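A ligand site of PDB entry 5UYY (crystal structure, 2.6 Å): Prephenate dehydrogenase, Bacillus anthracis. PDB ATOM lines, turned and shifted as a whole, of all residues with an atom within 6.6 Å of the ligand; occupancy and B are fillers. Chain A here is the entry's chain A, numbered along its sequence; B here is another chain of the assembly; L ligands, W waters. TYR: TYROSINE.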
ATOM      1  N   VAL A 316       1.668  -7.840 -24.850  1.00  0.00           N
ATOM      2  CA  VAL A 316       0.979  -6.638 -25.337  1.00  0.00           C
ATOM      3  C   VAL A 316       0.316  -5.830 -24.240  1.00  0.00           C
ATOM      4  O   VAL A 316      -0.004  -6.319 -23.178  1.00  0.00           O
ATOM      5  CB  VAL A 316      -0.133  -6.967 -26.335  1.00  0.00           C
ATOM      6  CG1 VAL A 316       0.410  -7.821 -27.434  1.00  0.00           C
ATOM      7  CG2 VAL A 316      -1.243  -7.709 -25.665  1.00  0.00           C
ATOM      8  N   LEU A 317       0.098  -4.565 -24.568  1.00  0.00           N
ATOM      9  CA  LEU A 317      -0.337  -3.561 -23.631  1.00  0.00           C
ATOM     10  C   LEU A 317      -1.841  -3.417 -23.709  1.00  0.00           C
ATOM     11  O   LEU A 317      -2.423  -3.515 -24.772  1.00  0.00           O
ATOM     12  CB  LEU A 317       0.311  -2.217 -23.955  1.00  0.00           C
ATOM     13  CG  LEU A 317       1.757  -1.941 -23.512  1.00  0.00           C
ATOM     14  CD1 LEU A 317       2.276  -0.691 -24.212  1.00  0.00           C
ATOM     15  CD2 LEU A 317       1.867  -1.761 -21.994  1.00  0.00           C
ATOM     16  N   ASP A 318      -2.466  -3.127 -22.566  1.00  0.00           N
ATOM     17  CA  ASP A 318      -3.879  -2.915 -22.562  1.00  0.00           C
ATOM     18  C   ASP A 318      -4.192  -1.477 -23.034  1.00  0.00           C
ATOM     19  O   ASP A 318      -4.496  -0.598 -22.234  1.00  0.00           O
ATOM     20  CB  ASP A 318      -4.470  -3.226 -21.178  1.00  0.00           C
ATOM     21  CG  ASP A 318      -5.984  -3.189 -21.160  1.00  0.00           C
ATOM     22  OD1 ASP A 318      -6.570  -3.162 -22.259  1.00  0.00           O
ATOM     23  OD2 ASP A 318      -6.563  -3.142 -20.071  1.00  0.00           O
ATOM     24  N   LYS A 319      -4.130  -1.267 -24.337  1.00  0.00           N
ATOM     25  CA  LYS A 319      -4.552   0.020 -24.937  1.00  0.00           C
ATOM     26  C   LYS A 319      -5.285  -0.199 -26.231  1.00  0.00           C
ATOM     27  O   LYS A 319      -5.175  -1.237 -26.877  1.00  0.00           O
ATOM     28  CB  LYS A 319      -3.378   0.976 -25.205  1.00  0.00           C
ATOM     29  CG  LYS A 319      -2.064   0.369 -25.663  1.00  0.00           C
ATOM     30  CD  LYS A 319      -1.129   1.434 -26.246  1.00  0.00           C
ATOM     31  CE  LYS A 319      -0.092   1.013 -27.330  1.00  0.00           C
ATOM     32  NZ  LYS A 319       0.486   2.186 -28.046  1.00  0.00           N
ATOM     33  N   VAL A 320      -6.037   0.809 -26.609  1.00  0.00           N
ATOM     34  CA  VAL A 320      -6.756   0.799 -27.836  1.00  0.00           C
ATOM     35  C   VAL A 320      -5.820   0.469 -29.004  1.00  0.00           C
ATOM     36  O   VAL A 320      -4.722   1.007 -29.135  1.00  0.00           O
ATOM     37  CB  VAL A 320      -7.417   2.167 -28.045  1.00  0.00           C
ATOM     38  CG1 VAL A 320      -7.932   2.309 -29.482  1.00  0.00           C
ATOM     39  CG2 VAL A 320      -8.556   2.355 -27.079  1.00  0.00           C
ATOM     40  N   GLY A 321      -6.224  -0.474 -29.840  1.00  0.00           N
ATOM     41  CA  GLY A 321      -5.459  -0.834 -31.029  1.00  0.00           C
ATOM     42  C   GLY A 321      -4.327  -1.840 -30.844  1.00  0.00           C
ATOM     43  O   GLY A 321      -3.663  -2.200 -31.806  1.00  0.00           O
ATOM     44  N   ALA A 322      -4.091  -2.328 -29.638  1.00  0.00           N
ATOM     45  CA  ALA A 322      -2.994  -3.303 -29.477  1.00  0.00           C
ATOM     46  C   ALA A 322      -3.225  -4.590 -30.310  1.00  0.00           C
ATOM     47  O   ALA A 322      -2.339  -5.050 -31.013  1.00  0.00           O
ATOM     48  CB  ALA A 322      -2.844  -3.646 -28.035  1.00  0.00           C
ATOM     49  N   LEU A 323      -4.437  -5.160 -30.211  1.00  0.00           N
ATOM     50  CA  LEU A 323      -4.790  -6.363 -30.975  1.00  0.00           C
ATOM     51  C   LEU A 323      -4.834  -6.136 -32.480  1.00  0.00           C
ATOM     52  O   LEU A 323      -4.322  -6.953 -33.249  1.00  0.00           O
ATOM     53  CB  LEU A 323      -6.146  -6.895 -30.523  1.00  0.00           C
ATOM     54  CG  LEU A 323      -6.081  -7.543 -29.144  1.00  0.00           C
ATOM     55  CD1 LEU A 323      -7.467  -7.829 -28.593  1.00  0.00           C
ATOM     56  CD2 LEU A 323      -5.296  -8.844 -29.229  1.00  0.00           C
ATOM     57  N   ALA A 324      -5.444  -5.016 -32.879  1.00  0.00           N
ATOM     58  CA  ALA A 324      -5.419  -4.526 -34.290  1.00  0.00           C
ATOM     59  C   ALA A 324      -4.041  -4.492 -34.874  1.00  0.00           C
ATOM     60  O   ALA A 324      -3.824  -4.935 -36.003  1.00  0.00           O
ATOM     61  CB  ALA A 324      -6.047  -3.154 -34.408  1.00  0.00           C
ATOM     62  N   ILE A 342      -6.725 -13.359 -24.365  1.00  0.00           N
ATOM     63  CA  ILE A 342      -5.957 -12.557 -23.427  1.00  0.00           C
ATOM     64  C   ILE A 342      -5.954 -13.272 -22.089  1.00  0.00           C
ATOM     65  O   ILE A 342      -7.010 -13.598 -21.531  1.00  0.00           O
ATOM     66  CB  ILE A 342      -6.590 -11.166 -23.266  1.00  0.00           C
ATOM     67  CG1 ILE A 342      -6.465 -10.331 -24.542  1.00  0.00           C
ATOM     68  CG2 ILE A 342      -6.054 -10.432 -22.038  1.00  0.00           C
ATOM     69  CD1 ILE A 342      -5.052  -9.889 -24.794  1.00  0.00           C
ATOM     70  N   LEU A 343      -4.781 -13.530 -21.553  1.00  0.00           N
ATOM     71  CA  LEU A 343      -4.605 -14.139 -20.260  1.00  0.00           C
ATOM     72  C   LEU A 343      -4.002 -13.013 -19.421  1.00  0.00           C
ATOM     73  O   LEU A 343      -3.026 -12.410 -19.841  1.00  0.00           O
ATOM     74  CB  LEU A 343      -3.658 -15.356 -20.324  1.00  0.00           C
ATOM     75  CG  LEU A 343      -3.629 -16.256 -21.577  1.00  0.00           C
ATOM     76  CD1 LEU A 343      -2.367 -17.089 -21.667  1.00  0.00           C
ATOM     77  CD2 LEU A 343      -4.793 -17.241 -21.636  1.00  0.00           C
ATOM     78  N   GLU A 344      -4.573 -12.716 -18.255  1.00  0.00           N
ATOM     79  CA  GLU A 344      -4.060 -11.605 -17.432  1.00  0.00           C
ATOM     80  C   GLU A 344      -2.924 -12.148 -16.527  1.00  0.00           C
ATOM     81  O   GLU A 344      -3.197 -12.670 -15.447  1.00  0.00           O
ATOM     82  CB  GLU A 344      -5.174 -10.944 -16.640  1.00  0.00           C
ATOM     83  CG  GLU A 344      -6.086 -10.012 -17.421  1.00  0.00           C
ATOM     84  CD  GLU A 344      -5.442  -8.848 -18.161  1.00  0.00           C
ATOM     85  OE1 GLU A 344      -4.394  -8.324 -17.700  1.00  0.00           O
ATOM     86  OE2 GLU A 344      -6.041  -8.422 -19.173  1.00  0.00           O
ATOM     87  N   GLY A 348       0.005  -4.710 -13.794  1.00  0.00           N
ATOM     88  CA  GLY A 348       0.424  -3.689 -14.711  1.00  0.00           C
ATOM     89  C   GLY A 348      -0.436  -3.691 -15.936  1.00  0.00           C
ATOM     90  O   GLY A 348      -1.367  -4.471 -16.053  1.00  0.00           O
ATOM     91  N   LEU A 349      -0.144  -2.785 -16.850  1.00  0.00           N
ATOM     92  CA  LEU A 349      -1.020  -2.655 -17.997  1.00  0.00           C
ATOM     93  C   LEU A 349      -0.755  -3.750 -19.043  1.00  0.00           C
ATOM     94  O   LEU A 349      -1.547  -3.929 -19.941  1.00  0.00           O
ATOM     95  CB  LEU A 349      -0.968  -1.244 -18.603  1.00  0.00           C
ATOM     96  CG  LEU A 349      -1.825  -0.154 -17.931  1.00  0.00           C
ATOM     97  CD1 LEU A 349      -1.569   1.155 -18.670  1.00  0.00           C
ATOM     98  CD2 LEU A 349      -3.311  -0.460 -17.873  1.00  0.00           C
ATOM     99  N   LEU A 350       0.357  -4.474 -18.933  1.00  0.00           N
ATOM    100  CA  LEU A 350       0.617  -5.639 -19.792  1.00  0.00           C
ATOM    101  C   LEU A 350      -0.350  -6.773 -19.511  1.00  0.00           C
ATOM    102  O   LEU A 350      -0.814  -6.946 -18.400  1.00  0.00           O
ATOM    103  CB  LEU A 350       2.065  -6.159 -19.664  1.00  0.00           C
ATOM    104  CG  LEU A 350       3.153  -5.253 -20.224  1.00  0.00           C
ATOM    105  CD1 LEU A 350       4.491  -5.874 -19.918  1.00  0.00           C
ATOM    106  CD2 LEU A 350       3.022  -5.035 -21.737  1.00  0.00           C
ATOM    107  N   GLY A 351      -0.670  -7.495 -20.599  1.00  0.00           N
ATOM    108  CA  GLY A 351      -1.399  -8.732 -20.633  1.00  0.00           C
ATOM    109  C   GLY A 351      -0.554  -9.605 -21.510  1.00  0.00           C
ATOM    110  O   GLY A 351       0.332  -9.134 -22.221  1.00  0.00           O
ATOM    111  N   VAL A 352      -0.822 -10.880 -21.420  1.00  0.00           N
ATOM    112  CA  VAL A 352      -0.327 -11.860 -22.349  1.00  0.00           C
ATOM    113  C   VAL A 352      -1.387 -12.291 -23.313  1.00  0.00           C
ATOM    114  O   VAL A 352      -2.458 -12.744 -22.962  1.00  0.00           O
ATOM    115  CB  VAL A 352       0.185 -13.092 -21.602  1.00  0.00           C
ATOM    116  CG1 VAL A 352       0.893 -13.961 -22.612  1.00  0.00           C
ATOM    117  CG2 VAL A 352       1.154 -12.636 -20.520  1.00  0.00           C
ATOM    118  N   LEU A 353      -1.050 -12.170 -24.571  1.00  0.00           N
ATOM    119  CA  LEU A 353      -1.928 -12.554 -25.659  1.00  0.00           C
ATOM    120  C   LEU A 353      -1.443 -13.893 -26.155  1.00  0.00           C
ATOM    121  O   LEU A 353      -0.293 -14.038 -26.524  1.00  0.00           O
ATOM    122  CB  LEU A 353      -1.842 -11.534 -26.796  1.00  0.00           C
ATOM    123  CG  LEU A 353      -2.583 -11.857 -28.095  1.00  0.00           C
ATOM    124  CD1 LEU A 353      -4.082 -11.909 -27.870  1.00  0.00           C
ATOM    125  CD2 LEU A 353      -2.258 -10.788 -29.107  1.00  0.00           C
ATOM    126  N   HIS B 141     -10.991  -6.270 -15.112  1.00  0.00           N
ATOM    127  CA  HIS B 141     -10.139  -7.337 -15.592  1.00  0.00           C
ATOM    128  C   HIS B 141      -8.717  -7.169 -15.005  1.00  0.00           C
ATOM    129  O   HIS B 141      -7.917  -8.124 -14.986  1.00  0.00           O
ATOM    130  CB  HIS B 141     -10.200  -7.399 -17.164  1.00  0.00           C
ATOM    131  CG  HIS B 141      -9.737  -6.148 -17.852  1.00  0.00           C
ATOM    132  ND1 HIS B 141     -10.478  -4.987 -17.780  1.00  0.00           N
ATOM    133  CD2 HIS B 141      -8.671  -5.854 -18.649  1.00  0.00           C
ATOM    134  CE1 HIS B 141      -9.890  -4.029 -18.473  1.00  0.00           C
ATOM    135  NE2 HIS B 141      -8.782  -4.521 -19.002  1.00  0.00           N
ATOM    136  N   LYS B 142      -8.387  -5.948 -14.551  1.00  0.00           N
ATOM    137  CA  LYS B 142      -7.053  -5.609 -13.997  1.00  0.00           C
ATOM    138  C   LYS B 142      -7.065  -5.371 -12.486  1.00  0.00           C
ATOM    139  O   LYS B 142      -8.129  -5.253 -11.925  1.00  0.00           O
ATOM    140  CB  LYS B 142      -6.553  -4.346 -14.629  1.00  0.00           C
ATOM    141  CG  LYS B 142      -6.347  -4.474 -16.103  1.00  0.00           C
ATOM    142  CD  LYS B 142      -5.090  -5.244 -16.424  1.00  0.00           C
ATOM    143  CE  LYS B 142      -4.629  -4.914 -17.819  1.00  0.00           C
ATOM    144  NZ  LYS B 142      -3.469  -5.766 -18.193  1.00  0.00           N
ATOM    145  N   THR B 327     -10.896  -5.990 -35.304  1.00  0.00           N
ATOM    146  CA  THR B 327     -10.214  -5.173 -34.297  1.00  0.00           C
ATOM    147  C   THR B 327      -9.861  -3.770 -34.840  1.00  0.00           C
ATOM    148  O   THR B 327      -9.869  -2.807 -34.067  1.00  0.00           O
ATOM    149  CB  THR B 327      -8.965  -5.833 -33.736  1.00  0.00           C
ATOM    150  OG1 THR B 327      -8.078  -6.193 -34.773  1.00  0.00           O
ATOM    151  CG2 THR B 327      -9.371  -7.082 -32.951  1.00  0.00           C
ATOM    152  N   ALA B 331     -10.858  -0.314 -32.798  1.00  0.00           N
ATOM    153  CA  ALA B 331      -9.771   0.610 -32.443  1.00  0.00           C
ATOM    154  C   ALA B 331      -9.987   1.978 -32.999  1.00  0.00           C
ATOM    155  O   ALA B 331      -9.706   2.999 -32.352  1.00  0.00           O
ATOM    156  CB  ALA B 331      -8.434   0.048 -32.894  1.00  0.00           C
ATOM    157  N   ILE B 335     -12.413   2.022 -28.842  1.00  0.00           N
ATOM    158  CA  ILE B 335     -12.884   1.044 -27.895  1.00  0.00           C
ATOM    159  C   ILE B 335     -11.767   0.080 -27.571  1.00  0.00           C
ATOM    160  O   ILE B 335     -11.180  -0.580 -28.466  1.00  0.00           O
ATOM    161  CB  ILE B 335     -14.059   0.224 -28.435  1.00  0.00           C
ATOM    162  CG1 ILE B 335     -15.187   1.166 -28.888  1.00  0.00           C
ATOM    163  CG2 ILE B 335     -14.575  -0.693 -27.379  1.00  0.00           C
ATOM    164  CD1 ILE B 335     -16.257   0.486 -29.719  1.00  0.00           C
ATOM    165  N   SER B 336     -11.528  -0.051 -26.279  1.00  0.00           N
ATOM    166  CA  SER B 336     -10.595  -1.036 -25.742  1.00  0.00           C
ATOM    167  C   SER B 336     -11.266  -2.394 -25.478  1.00  0.00           C
ATOM    168  O   SER B 336     -12.343  -2.470 -24.943  1.00  0.00           O
ATOM    169  CB  SER B 336     -10.000  -0.513 -24.460  1.00  0.00           C
ATOM    170  OG  SER B 336      -8.805  -1.194 -24.217  1.00  0.00           O
ATOM    171  N   ILE B 337     -10.644  -3.452 -25.928  1.00  0.00           N
ATOM    172  CA  ILE B 337     -11.196  -4.820 -25.837  1.00  0.00           C
ATOM    173  C   ILE B 337     -10.592  -5.448 -24.587  1.00  0.00           C
ATOM    174  O   ILE B 337      -9.374  -5.464 -24.444  1.00  0.00           O
ATOM    175  CB  ILE B 337     -10.779  -5.661 -27.083  1.00  0.00           C
ATOM    176  CG1 ILE B 337     -11.558  -5.202 -28.275  1.00  0.00           C
ATOM    177  CG2 ILE B 337     -11.040  -7.159 -26.933  1.00  0.00           C
ATOM    178  CD1 ILE B 337     -10.971  -5.748 -29.601  1.00  0.00           C
ATOM    179  N   THR B 338     -11.402  -6.092 -23.764  1.00  0.00           N
ATOM    180  CA  THR B 338     -10.810  -6.798 -22.623  1.00  0.00           C
ATOM    181  C   THR B 338     -10.402  -8.209 -22.968  1.00  0.00           C
ATOM    182  O   THR B 338      -9.427  -8.735 -22.463  1.00  0.00           O
ATOM    183  CB  THR B 338     -11.735  -6.833 -21.415  1.00  0.00           C
ATOM    184  OG1 THR B 338     -12.957  -7.425 -21.806  1.00  0.00           O
ATOM    185  CG2 THR B 338     -12.049  -5.423 -20.974  1.00  0.00           C
ATOM    186  N   ASN B 339     -11.180  -8.841 -23.824  1.00  0.00           N
ATOM    187  CA  ASN B 339     -10.840 -10.177 -24.325  1.00  0.00           C
ATOM    188  C   ASN B 339     -11.520 -10.515 -25.598  1.00  0.00           C
ATOM    189  O   ASN B 339     -12.463  -9.864 -26.017  1.00  0.00           O
ATOM    190  CB  ASN B 339     -11.165 -11.274 -23.303  1.00  0.00           C
ATOM    191  CG  ASN B 339     -10.086 -12.341 -23.222  1.00  0.00           C
ATOM    192  OD1 ASN B 339      -9.592 -12.843 -24.208  1.00  0.00           O
ATOM    193  ND2 ASN B 339      -9.680 -12.649 -22.011  1.00  0.00           N
ATOM    194  N   GLN B 358     -15.186  -3.678 -21.368  1.00  0.00           N
ATOM    195  CA  GLN B 358     -15.079  -3.199 -19.975  1.00  0.00           C
ATOM    196  C   GLN B 358     -16.409  -2.770 -19.430  1.00  0.00           C
ATOM    197  O   GLN B 358     -16.611  -2.900 -18.254  1.00  0.00           O
ATOM    198  CB  GLN B 358     -14.131  -1.970 -19.829  1.00  0.00           C
ATOM    199  CG  GLN B 358     -12.706  -2.243 -20.272  1.00  0.00           C
ATOM    200  CD  GLN B 358     -11.808  -1.007 -20.316  1.00  0.00           C
ATOM    201  OE1 GLN B 358     -11.977  -0.064 -19.563  1.00  0.00           O
ATOM    202  NE2 GLN B 358     -10.826  -1.048 -21.181  1.00  0.00           N
HETATM  203  N   TYR L   1      -7.338  -3.416 -24.784  1.00  0.00           N
HETATM  204  CA  TYR L   1      -6.476  -3.986 -25.855  1.00  0.00           C
HETATM  205  C   TYR L   1      -7.101  -3.716 -27.224  1.00  0.00           C
HETATM  206  O   TYR L   1      -6.461  -4.081 -28.212  1.00  0.00           O
HETATM  207  CB  TYR L   1      -6.246  -5.487 -25.680  1.00  0.00           C
HETATM  208  CG  TYR L   1      -5.665  -5.895 -24.341  1.00  0.00           C
HETATM  209  CD1 TYR L   1      -6.493  -6.184 -23.255  1.00  0.00           C
HETATM  210  CD2 TYR L   1      -4.287  -6.031 -24.172  1.00  0.00           C
HETATM  211  CE1 TYR L   1      -5.987  -6.559 -22.034  1.00  0.00           C
HETATM  212  CE2 TYR L   1      -3.764  -6.430 -22.938  1.00  0.00           C
HETATM  213  CZ  TYR L   1      -4.624  -6.682 -21.869  1.00  0.00           C
HETATM  214  OH  TYR L   1      -4.131  -7.056 -20.643  1.00  0.00           O
HETATM  215  OXT TYR L   1      -8.183  -3.118 -27.351  1.00  0.00           O
HETATM  216  O   HOH W   1      -7.122  -3.461 -30.873  1.00  0.00           O
HETATM  217  O   HOH W   2      -8.744  -1.455 -29.329  1.00  0.00           O
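Water W2 lies within hydrogen-bond range of OXT of the ligand (2.6 Å), O of Ile 335 of chain B (2.7 Å) and N of Gly 321 (2.8 Å).
An oxygen (O) of the ligand sits close to the backbone carbonyl oxygen (O) of Lys 319 (3.4 Å).
Merely in contact with the ligand: Leu 317 (3.2 Å), Val 316 (3.8 Å), Ile 342 (3.9 Å), Leu 350 (3.96 Å), Gly 321 (3.96 Å) and Thr 338 of chain B (3.97 Å).
OD1 of Asp 318 lies within salt-bridge range of N of the ligand, 2.7 Å away.
The side-chain hydroxyl (OG) of Ser 336 of chain B lies within hydrogen-bond range of a nitrogen (N) of the ligand (2.7 Å).
The side-chain carboxylate of Glu 344 is in hydrogen-bond range of an oxygen (OH) of the ligand.
The side-chain amino group (NZ) of Lys 142 of chain B sits at hydrogen-bond distance from an oxygen (OH) of the ligand (2.8 Å).
The backbone NH of Ile 337 of chain B is in hydrogen-bond range of an oxygen (OXT) of the ligand (2.9 Å).
A nitrogen (N) of the ligand lies within hydrogen-bond range of the backbone carbonyl oxygen of Ile 337 of chain B, at 2.9 Å.
N of Leu 323 lies within hydrogen-bond range of O of the ligand, 3.0 Å away.
The backbone NH of Gly 351 sits close to an oxygen (OH) of the ligand, at 3.5 Å.
The backbone NH of Ala 322 lies within hydrogen-bond range of an oxygen (O) of the ligand (3.3 Å).
The backbone carbonyl oxygen (O) of Leu 349 lies within hydrogen-bond range of the backbone NH (N) of Asp 318 (2.9 Å).
NE2 of His 141 of chain B sits at hydrogen-bond distance from OD2 of Asp 318, 2.8 Å away.
OE1 of Glu 344 lies within salt-bridge range of NZ of Lys 142 of chain B (2.8 Å).
The side-chain amino group (NZ) of Lys 142 of chain B sits at hydrogen-bond distance from the backbone carbonyl oxygen (O) of Leu 350 (2.9 Å).
NZ of Lys 142 of chain B sits at hydrogen-bond distance from O of Leu 349 (3.2 Å).
The backbone carbonyl oxygen (O) of Gly 348 sits at hydrogen-bond distance from the side-chain amino group (NZ) of Lys 142 of chain B (3.3 Å).
N of Gly 351 sits at hydrogen-bond distance from O of Val 316.
The side-chain amide nitrogen (ND2) of Asn 339 of chain B sits at hydrogen-bond distance from the backbone carbonyl oxygen (O) of Ile 342 (2.9 Å).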
